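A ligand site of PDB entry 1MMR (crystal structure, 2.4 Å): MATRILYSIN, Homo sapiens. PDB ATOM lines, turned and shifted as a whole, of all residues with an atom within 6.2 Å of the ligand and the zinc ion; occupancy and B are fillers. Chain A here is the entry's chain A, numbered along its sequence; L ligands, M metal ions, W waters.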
ATOM      1  N   ASP A  76      20.385  32.226   5.916  1.00  0.00           N
ATOM      2  CA  ASP A  76      20.356  31.686   7.267  1.00  0.00           C
ATOM      3  C   ASP A  76      21.192  32.350   8.303  1.00  0.00           C
ATOM      4  O   ASP A  76      21.551  31.691   9.266  1.00  0.00           O
ATOM      5  CB  ASP A  76      20.761  30.191   7.105  1.00  0.00           C
ATOM      6  CG  ASP A  76      22.131  30.090   6.442  1.00  0.00           C
ATOM      7  OD1 ASP A  76      22.798  31.092   6.264  1.00  0.00           O
ATOM      8  OD2 ASP A  76      22.564  29.013   6.052  1.00  0.00           O
ATOM      9  N   GLY A  79      27.465  32.336   8.778  1.00  0.00           N
ATOM     10  CA  GLY A  79      27.816  30.918   8.619  1.00  0.00           C
ATOM     11  C   GLY A  79      26.889  30.112   7.748  1.00  0.00           C
ATOM     12  O   GLY A  79      25.985  30.651   7.105  1.00  0.00           O
ATOM     13  N   ASN A  80      27.161  28.816   7.641  1.00  0.00           N
ATOM     14  CA  ASN A  80      26.390  27.866   6.828  1.00  0.00           C
ATOM     15  C   ASN A  80      26.319  28.339   5.390  1.00  0.00           C
ATOM     16  O   ASN A  80      27.392  28.513   4.824  1.00  0.00           O
ATOM     17  CB  ASN A  80      25.027  27.704   7.471  1.00  0.00           C
ATOM     18  CG  ASN A  80      25.135  26.905   8.741  1.00  0.00           C
ATOM     19  OD1 ASN A  80      24.127  26.535   9.322  1.00  0.00           O
ATOM     20  ND2 ASN A  80      26.305  26.555   9.281  1.00  0.00           N
ATOM     21  N   THR A  81      25.180  28.541   4.721  1.00  0.00           N
ATOM     22  CA  THR A  81      25.187  29.007   3.338  1.00  0.00           C
ATOM     23  C   THR A  81      25.705  30.410   3.286  1.00  0.00           C
ATOM     24  O   THR A  81      25.170  31.307   3.955  1.00  0.00           O
ATOM     25  CB  THR A  81      23.755  28.990   2.752  1.00  0.00           C
ATOM     26  OG1 THR A  81      23.250  27.666   2.950  1.00  0.00           O
ATOM     27  CG2 THR A  81      23.722  29.376   1.257  1.00  0.00           C
ATOM     28  N   LEU A  82      26.773  30.629   2.566  1.00  0.00           N
ATOM     29  CA  LEU A  82      27.373  31.975   2.399  1.00  0.00           C
ATOM     30  C   LEU A  82      26.722  32.802   1.295  1.00  0.00           C
ATOM     31  O   LEU A  82      26.697  34.022   1.353  1.00  0.00           O
ATOM     32  CB  LEU A  82      28.866  31.821   2.050  1.00  0.00           C
ATOM     33  CG  LEU A  82      29.935  31.576   3.120  1.00  0.00           C
ATOM     34  CD1 LEU A  82      29.352  31.125   4.440  1.00  0.00           C
ATOM     35  CD2 LEU A  82      30.966  30.650   2.451  1.00  0.00           C
ATOM     36  N   ALA A  83      26.256  32.140   0.244  1.00  0.00           N
ATOM     37  CA  ALA A  83      25.674  32.782  -0.930  1.00  0.00           C
ATOM     38  C   ALA A  83      24.978  31.713  -1.766  1.00  0.00           C
ATOM     39  O   ALA A  83      24.963  30.564  -1.309  1.00  0.00           O
ATOM     40  CB  ALA A  83      26.827  33.409  -1.708  1.00  0.00           C
ATOM     41  N   HIS A  84      24.304  32.055  -2.880  1.00  0.00           N
ATOM     42  CA  HIS A  84      23.693  31.045  -3.778  1.00  0.00           C
ATOM     43  C   HIS A  84      23.454  31.704  -5.155  1.00  0.00           C
ATOM     44  O   HIS A  84      23.192  32.918  -5.261  1.00  0.00           O
ATOM     45  CB  HIS A  84      22.316  30.431  -3.253  1.00  0.00           C
ATOM     46  CG  HIS A  84      21.226  31.408  -2.843  1.00  0.00           C
ATOM     47  ND1 HIS A  84      20.542  31.283  -1.717  1.00  0.00           N
ATOM     48  CD2 HIS A  84      20.806  32.538  -3.497  1.00  0.00           C
ATOM     49  CE1 HIS A  84      19.729  32.293  -1.637  1.00  0.00           C
ATOM     50  NE2 HIS A  84      19.900  33.039  -2.705  1.00  0.00           N
ATOM     51  N   ALA A  85      23.559  30.931  -6.221  1.00  0.00           N
ATOM     52  CA  ALA A  85      23.381  31.465  -7.588  1.00  0.00           C
ATOM     53  C   ALA A  85      22.491  30.512  -8.364  1.00  0.00           C
ATOM     54  O   ALA A  85      22.336  29.361  -7.945  1.00  0.00           O
ATOM     55  CB  ALA A  85      24.738  31.576  -8.335  1.00  0.00           C
ATOM     56  N   ILE A 112      34.917  36.170   5.047  1.00  0.00           N
ATOM     57  CA  ILE A 112      34.774  35.360   3.829  1.00  0.00           C
ATOM     58  C   ILE A 112      35.315  36.165   2.673  1.00  0.00           C
ATOM     59  O   ILE A 112      34.906  37.311   2.482  1.00  0.00           O
ATOM     60  CB  ILE A 112      33.280  35.002   3.619  1.00  0.00           C
ATOM     61  CG1 ILE A 112      32.698  34.303   4.877  1.00  0.00           C
ATOM     62  CG2 ILE A 112      33.155  34.031   2.423  1.00  0.00           C
ATOM     63  CD1 ILE A 112      33.261  32.906   5.208  1.00  0.00           C
ATOM     64  N   TYR A 116      36.832  34.996  -4.007  1.00  0.00           N
ATOM     65  CA  TYR A 116      36.676  33.543  -4.091  1.00  0.00           C
ATOM     66  C   TYR A 116      35.188  33.187  -4.173  1.00  0.00           C
ATOM     67  O   TYR A 116      34.775  32.472  -5.093  1.00  0.00           O
ATOM     68  CB  TYR A 116      37.339  32.896  -2.845  1.00  0.00           C
ATOM     69  CG  TYR A 116      37.332  31.420  -3.037  1.00  0.00           C
ATOM     70  CD1 TYR A 116      36.209  30.669  -2.658  1.00  0.00           C
ATOM     71  CD2 TYR A 116      38.432  30.783  -3.642  1.00  0.00           C
ATOM     72  CE1 TYR A 116      36.172  29.286  -2.883  1.00  0.00           C
ATOM     73  CE2 TYR A 116      38.408  29.395  -3.868  1.00  0.00           C
ATOM     74  CZ  TYR A 116      37.281  28.651  -3.483  1.00  0.00           C
ATOM     75  OH  TYR A 116      37.310  27.273  -3.589  1.00  0.00           O
ATOM     76  N   ALA A 117      34.362  33.685  -3.239  1.00  0.00           N
ATOM     77  CA  ALA A 117      32.900  33.418  -3.232  1.00  0.00           C
ATOM     78  C   ALA A 117      32.264  33.873  -4.553  1.00  0.00           C
ATOM     79  O   ALA A 117      31.438  33.185  -5.149  1.00  0.00           O
ATOM     80  CB  ALA A 117      32.200  34.178  -2.080  1.00  0.00           C
ATOM     81  N   ALA A 118      32.622  35.038  -5.046  1.00  0.00           N
ATOM     82  CA  ALA A 118      32.069  35.498  -6.326  1.00  0.00           C
ATOM     83  C   ALA A 118      32.525  34.566  -7.451  1.00  0.00           C
ATOM     84  O   ALA A 118      31.746  34.264  -8.344  1.00  0.00           O
ATOM     85  CB  ALA A 118      32.545  36.944  -6.668  1.00  0.00           C
ATOM     86  N   HIS A 120      33.057  31.350  -7.414  1.00  0.00           N
ATOM     87  CA  HIS A 120      32.213  30.149  -7.286  1.00  0.00           C
ATOM     88  C   HIS A 120      30.748  30.435  -7.723  1.00  0.00           C
ATOM     89  O   HIS A 120      30.142  29.699  -8.517  1.00  0.00           O
ATOM     90  CB  HIS A 120      32.304  29.699  -5.807  1.00  0.00           C
ATOM     91  CG  HIS A 120      31.511  28.417  -5.532  1.00  0.00           C
ATOM     92  ND1 HIS A 120      32.045  27.225  -5.435  1.00  0.00           N
ATOM     93  CD2 HIS A 120      30.156  28.314  -5.359  1.00  0.00           C
ATOM     94  CE1 HIS A 120      31.078  26.382  -5.213  1.00  0.00           C
ATOM     95  NE2 HIS A 120      29.963  27.040  -5.176  1.00  0.00           N
ATOM     96  N   GLU A 121      30.143  31.477  -7.172  1.00  0.00           N
ATOM     97  CA  GLU A 121      28.788  31.848  -7.504  1.00  0.00           C
ATOM     98  C   GLU A 121      28.669  32.200  -8.969  1.00  0.00           C
ATOM     99  O   GLU A 121      27.729  31.774  -9.630  1.00  0.00           O
ATOM    100  CB  GLU A 121      28.336  33.049  -6.670  1.00  0.00           C
ATOM    101  CG  GLU A 121      28.160  32.829  -5.156  1.00  0.00           C
ATOM    102  CD  GLU A 121      27.737  31.392  -4.765  1.00  0.00           C
ATOM    103  OE1 GLU A 121      26.679  30.905  -5.151  1.00  0.00           O
ATOM    104  OE2 GLU A 121      28.506  30.756  -4.051  1.00  0.00           O
ATOM    105  N   HIS A 124      28.408  29.192 -11.119  1.00  0.00           N
ATOM    106  CA  HIS A 124      27.028  28.699 -11.190  1.00  0.00           C
ATOM    107  C   HIS A 124      26.235  29.579 -12.168  1.00  0.00           C
ATOM    108  O   HIS A 124      25.513  29.054 -13.018  1.00  0.00           O
ATOM    109  CB  HIS A 124      26.311  28.761  -9.786  1.00  0.00           C
ATOM    110  CG  HIS A 124      26.740  27.647  -8.853  1.00  0.00           C
ATOM    111  ND1 HIS A 124      26.761  26.353  -9.147  1.00  0.00           N
ATOM    112  CD2 HIS A 124      27.076  27.790  -7.526  1.00  0.00           C
ATOM    113  CE1 HIS A 124      27.090  25.703  -8.057  1.00  0.00           C
ATOM    114  NE2 HIS A 124      27.278  26.555  -7.094  1.00  0.00           N
ATOM    115  N   HIS A 130      28.625  21.573  -9.130  1.00  0.00           N
ATOM    116  CA  HIS A 130      29.653  21.281  -8.141  1.00  0.00           C
ATOM    117  C   HIS A 130      30.625  20.215  -8.567  1.00  0.00           C
ATOM    118  O   HIS A 130      30.311  19.251  -9.304  1.00  0.00           O
ATOM    119  CB  HIS A 130      29.011  20.854  -6.827  1.00  0.00           C
ATOM    120  CG  HIS A 130      28.466  22.076  -6.095  1.00  0.00           C
ATOM    121  ND1 HIS A 130      27.458  22.081  -5.235  1.00  0.00           N
ATOM    122  CD2 HIS A 130      29.029  23.341  -6.096  1.00  0.00           C
ATOM    123  CE1 HIS A 130      27.395  23.287  -4.714  1.00  0.00           C
ATOM    124  NE2 HIS A 130      28.336  24.030  -5.230  1.00  0.00           N
ATOM    125  N   VAL A 137      37.599  25.288  -7.591  1.00  0.00           N
ATOM    126  CA  VAL A 137      36.843  26.444  -7.070  1.00  0.00           C
ATOM    127  C   VAL A 137      35.378  26.012  -6.925  1.00  0.00           C
ATOM    128  O   VAL A 137      34.659  26.434  -6.008  1.00  0.00           O
ATOM    129  CB  VAL A 137      36.970  27.641  -8.065  1.00  0.00           C
ATOM    130  CG1 VAL A 137      36.127  28.866  -7.613  1.00  0.00           C
ATOM    131  CG2 VAL A 137      38.472  28.036  -8.151  1.00  0.00           C
ATOM    132  N   MET A 138      34.884  25.176  -7.827  1.00  0.00           N
ATOM    133  CA  MET A 138      33.485  24.734  -7.743  1.00  0.00           C
ATOM    134  C   MET A 138      33.213  23.645  -6.714  1.00  0.00           C
ATOM    135  O   MET A 138      32.140  23.022  -6.716  1.00  0.00           O
ATOM    136  CB  MET A 138      33.009  24.311  -9.130  1.00  0.00           C
ATOM    137  CG  MET A 138      32.931  25.513 -10.130  1.00  0.00           C
ATOM    138  SD  MET A 138      32.025  26.995  -9.607  1.00  0.00           S
ATOM    139  CE  MET A 138      30.441  26.247  -9.147  1.00  0.00           C
ATOM    140  N   TYR A 139      34.169  23.365  -5.817  1.00  0.00           N
ATOM    141  CA  TYR A 139      33.891  22.356  -4.769  1.00  0.00           C
ATOM    142  C   TYR A 139      32.792  22.986  -3.880  1.00  0.00           C
ATOM    143  O   TYR A 139      32.763  24.211  -3.721  1.00  0.00           O
ATOM    144  CB  TYR A 139      35.161  22.104  -3.947  1.00  0.00           C
ATOM    145  CG  TYR A 139      35.040  20.868  -3.154  1.00  0.00           C
ATOM    146  CD1 TYR A 139      34.942  19.604  -3.784  1.00  0.00           C
ATOM    147  CD2 TYR A 139      34.998  20.978  -1.759  1.00  0.00           C
ATOM    148  CE1 TYR A 139      34.800  18.442  -3.011  1.00  0.00           C
ATOM    149  CE2 TYR A 139      34.853  19.823  -0.981  1.00  0.00           C
ATOM    150  CZ  TYR A 139      34.750  18.565  -1.605  1.00  0.00           C
ATOM    151  OH  TYR A 139      34.560  17.448  -0.802  1.00  0.00           O
ATOM    152  N   PRO A 140      31.836  22.226  -3.300  1.00  0.00           N
ATOM    153  CA  PRO A 140      30.746  22.840  -2.492  1.00  0.00           C
ATOM    154  C   PRO A 140      31.057  23.639  -1.215  1.00  0.00           C
ATOM    155  O   PRO A 140      30.282  24.524  -0.797  1.00  0.00           O
ATOM    156  CB  PRO A 140      29.810  21.667  -2.236  1.00  0.00           C
ATOM    157  CG  PRO A 140      30.684  20.449  -2.452  1.00  0.00           C
ATOM    158  CD  PRO A 140      31.494  20.850  -3.651  1.00  0.00           C
ATOM    159  N   THR A 141      32.125  23.320  -0.506  1.00  0.00           N
ATOM    160  CA  THR A 141      32.478  24.041   0.724  1.00  0.00           C
ATOM    161  C   THR A 141      33.632  25.005   0.550  1.00  0.00           C
ATOM    162  O   THR A 141      34.485  24.878  -0.351  1.00  0.00           O
ATOM    163  CB  THR A 141      32.773  22.971   1.748  1.00  0.00           C
ATOM    164  OG1 THR A 141      33.752  22.078   1.194  1.00  0.00           O
ATOM    165  CG2 THR A 141      31.513  22.146   2.093  1.00  0.00           C
ATOM    166  N   TYR A 142      33.675  26.004   1.405  1.00  0.00           N
ATOM    167  CA  TYR A 142      34.705  27.051   1.444  1.00  0.00           C
ATOM    168  C   TYR A 142      35.903  26.659   2.298  1.00  0.00           C
ATOM    169  O   TYR A 142      35.740  25.987   3.312  1.00  0.00           O
ATOM    170  CB  TYR A 142      34.038  28.289   2.021  1.00  0.00           C
ATOM    171  CG  TYR A 142      34.898  29.455   2.114  1.00  0.00           C
ATOM    172  CD1 TYR A 142      35.024  30.296   0.997  1.00  0.00           C
ATOM    173  CD2 TYR A 142      35.588  29.706   3.312  1.00  0.00           C
ATOM    174  CE1 TYR A 142      35.852  31.420   1.084  1.00  0.00           C
ATOM    175  CE2 TYR A 142      36.412  30.841   3.380  1.00  0.00           C
ATOM    176  CZ  TYR A 142      36.542  31.691   2.273  1.00  0.00           C
ATOM    177  OH  TYR A 142      37.352  32.810   2.351  1.00  0.00           O
ATOM    178  N   GLY A 143      37.097  27.118   1.971  1.00  0.00           N
ATOM    179  CA  GLY A 143      38.273  26.846   2.834  1.00  0.00           C
ATOM    180  C   GLY A 143      39.258  25.740   2.543  1.00  0.00           C
ATOM    181  O   GLY A 143      40.273  25.670   3.233  1.00  0.00           O
HETATM  182  S1  LIG L   1      26.543  27.435  -2.731  1.00  0.00           S
HETATM  183  N1  LIG L   1      27.200  26.088  -3.302  1.00  0.00           N
HETATM  184  N2  LIG L   1      26.289  28.194  -4.103  1.00  0.00           N
HETATM  185  C1  LIG L   1      27.555  28.584  -1.909  1.00  0.00           C
HETATM  186  C2  LIG L   1      28.732  27.952  -1.144  1.00  0.00           C
HETATM  187  C3  LIG L   1      28.468  27.726   0.342  1.00  0.00           C
HETATM  188  O1  LIG L   1      27.837  28.547   1.013  1.00  0.00           O
HETATM  189  N3  LIG L   1      28.968  26.630   0.907  1.00  0.00           N
HETATM  190  C4  LIG L   1      28.793  26.354   2.328  1.00  0.00           C
HETATM  191  C5  LIG L   1      30.060  26.695   3.089  1.00  0.00           C
HETATM  192  O2  LIG L   1      31.165  26.351   2.675  1.00  0.00           O
HETATM  193  N4  LIG L   1      29.915  27.389   4.209  1.00  0.00           N
HETATM  194  C6  LIG L   1      31.041  27.753   5.082  1.00  0.00           C
HETATM  195  C7  LIG L   1      30.455  28.066   6.487  1.00  0.00           C
HETATM  196  C8  LIG L   1      30.868  27.054   7.566  1.00  0.00           C
HETATM  197  C9  LIG L   1      29.953  25.850   7.606  1.00  0.00           C
HETATM  198  C10 LIG L   1      30.731  24.521   7.693  1.00  0.00           C
HETATM  199  C11 LIG L   1      29.854  23.350   7.190  1.00  0.00           C
HETATM  200  N5  LIG L   1      29.017  23.734   6.017  1.00  0.00           N
HETATM  201  C12 LIG L   1      29.857  29.015  -1.288  1.00  0.00           C
HETATM  202  C13 LIG L   1      31.349  28.685  -1.190  1.00  0.00           C
HETATM  203  C14 LIG L   1      31.745  27.355  -1.866  1.00  0.00           C
HETATM  204  C15 LIG L   1      32.037  29.861  -1.923  1.00  0.00           C
HETATM  205  C16 LIG L   1      28.425  24.873   2.511  1.00  0.00           C
HETATM  206  C17 LIG L   1      28.359  24.476   3.958  1.00  0.00           C
HETATM  207  C18 LIG L   1      29.433  24.047   4.760  1.00  0.00           C
HETATM  208  C19 LIG L   1      27.231  24.412   4.793  1.00  0.00           C
HETATM  209  C20 LIG L   1      27.678  23.952   6.061  1.00  0.00           C
HETATM  210  C21 LIG L   1      25.882  24.705   4.585  1.00  0.00           C
HETATM  211  C22 LIG L   1      26.766  23.782   7.116  1.00  0.00           C
HETATM  212  C23 LIG L   1      24.983  24.530   5.639  1.00  0.00           C
HETATM  213  C24 LIG L   1      25.414  24.072   6.891  1.00  0.00           C
HETATM  214  C25 LIG L   1      25.015  27.231  -1.891  1.00  0.00           C
HETATM  215 ZN    ZN M   1      28.019  26.101  -5.123  1.00  0.00          ZN
HETATM  216  O   HOH W   1      28.962  28.455  10.036  1.00  0.00           O
HETATM  217  O   HOH W   2      27.315  24.350  -1.375  1.00  0.00           O
HETATM  218  O   HOH W   3      23.920  27.851  -5.477  1.00  0.00           O
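N of Ala 85 is in hydrogen-bond range of OE1 of Glu 121, at 3.3 Å. A ring nitrogen (ND1) of His 120 lies within hydrogen-bond range of the backbone carbonyl oxygen (O) of Val 137, at 2.8 Å. OE1 of Glu 121 lies close to N of His 84, 3.5 Å away.
Water W3 lies within hydrogen-bond range of a nitrogen (N2) of the ligand (2.8 Å) and the backbone NH (N) of Ala 85 (3.2 Å).
The backbone NH (N) of Tyr 142 is in hydrogen-bond range of an oxygen (O2) of the ligand. A nitrogen (N4) of the ligand is in hydrogen-bond range of the backbone carbonyl oxygen (O) of Asn 80 (2.8 Å). O1 of the ligand sits at hydrogen-bond distance from N of Leu 82 (2.8 Å). A nitrogen (N2) of the ligand lies within hydrogen-bond range of the side-chain carboxylate (OE1) of Glu 121, at 2.9 Å. A nitrogen (N3) of the ligand lies within hydrogen-bond range of the backbone carbonyl oxygen (O) of Pro 140 (3.0 Å).
The zinc ion is bound by a nitrogen (N1) of the ligand, a ring nitrogen (NE2) of His 130, a ring nitrogen (NE2) of His 124 and a ring nitrogen (NE2) of His 120. The zinc ion has four donor atoms within binding distance.
Three residues have an atom within 4 Å of the zinc ion: His 120, His 124 and His 130.
The backbone carbonyl oxygen of Ala 83 lies close to a sulfur (S1) of the ligand, 3.8 Å away. Thr 81 touches the ligand. CA of His 84 touches N2 of the ligand (3.9 Å). Ala 117 touches the ligand (CA to C15, 3.9 Å). Tyr 139 touches the ligand (O to C14, 3.8 Å). CA of Thr 141 touches O2 of the ligand, at 3.3 Å. Hydrophobic or aromatic side chains within 4 Å of the ligand: Leu 82, His 120, His 124, His 130 and Tyr 142. Within 4 Å of the ligand: Asn 80, Thr 81, Leu 82, Ala 83, His 84, Ala 117, His 120, Glu 121, His 124, His 130, Tyr 139, Pro 140, Thr 141 and Tyr 142. The nearest printed residue that does not touch the ligand is Tyr 116 (4.3 Å).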
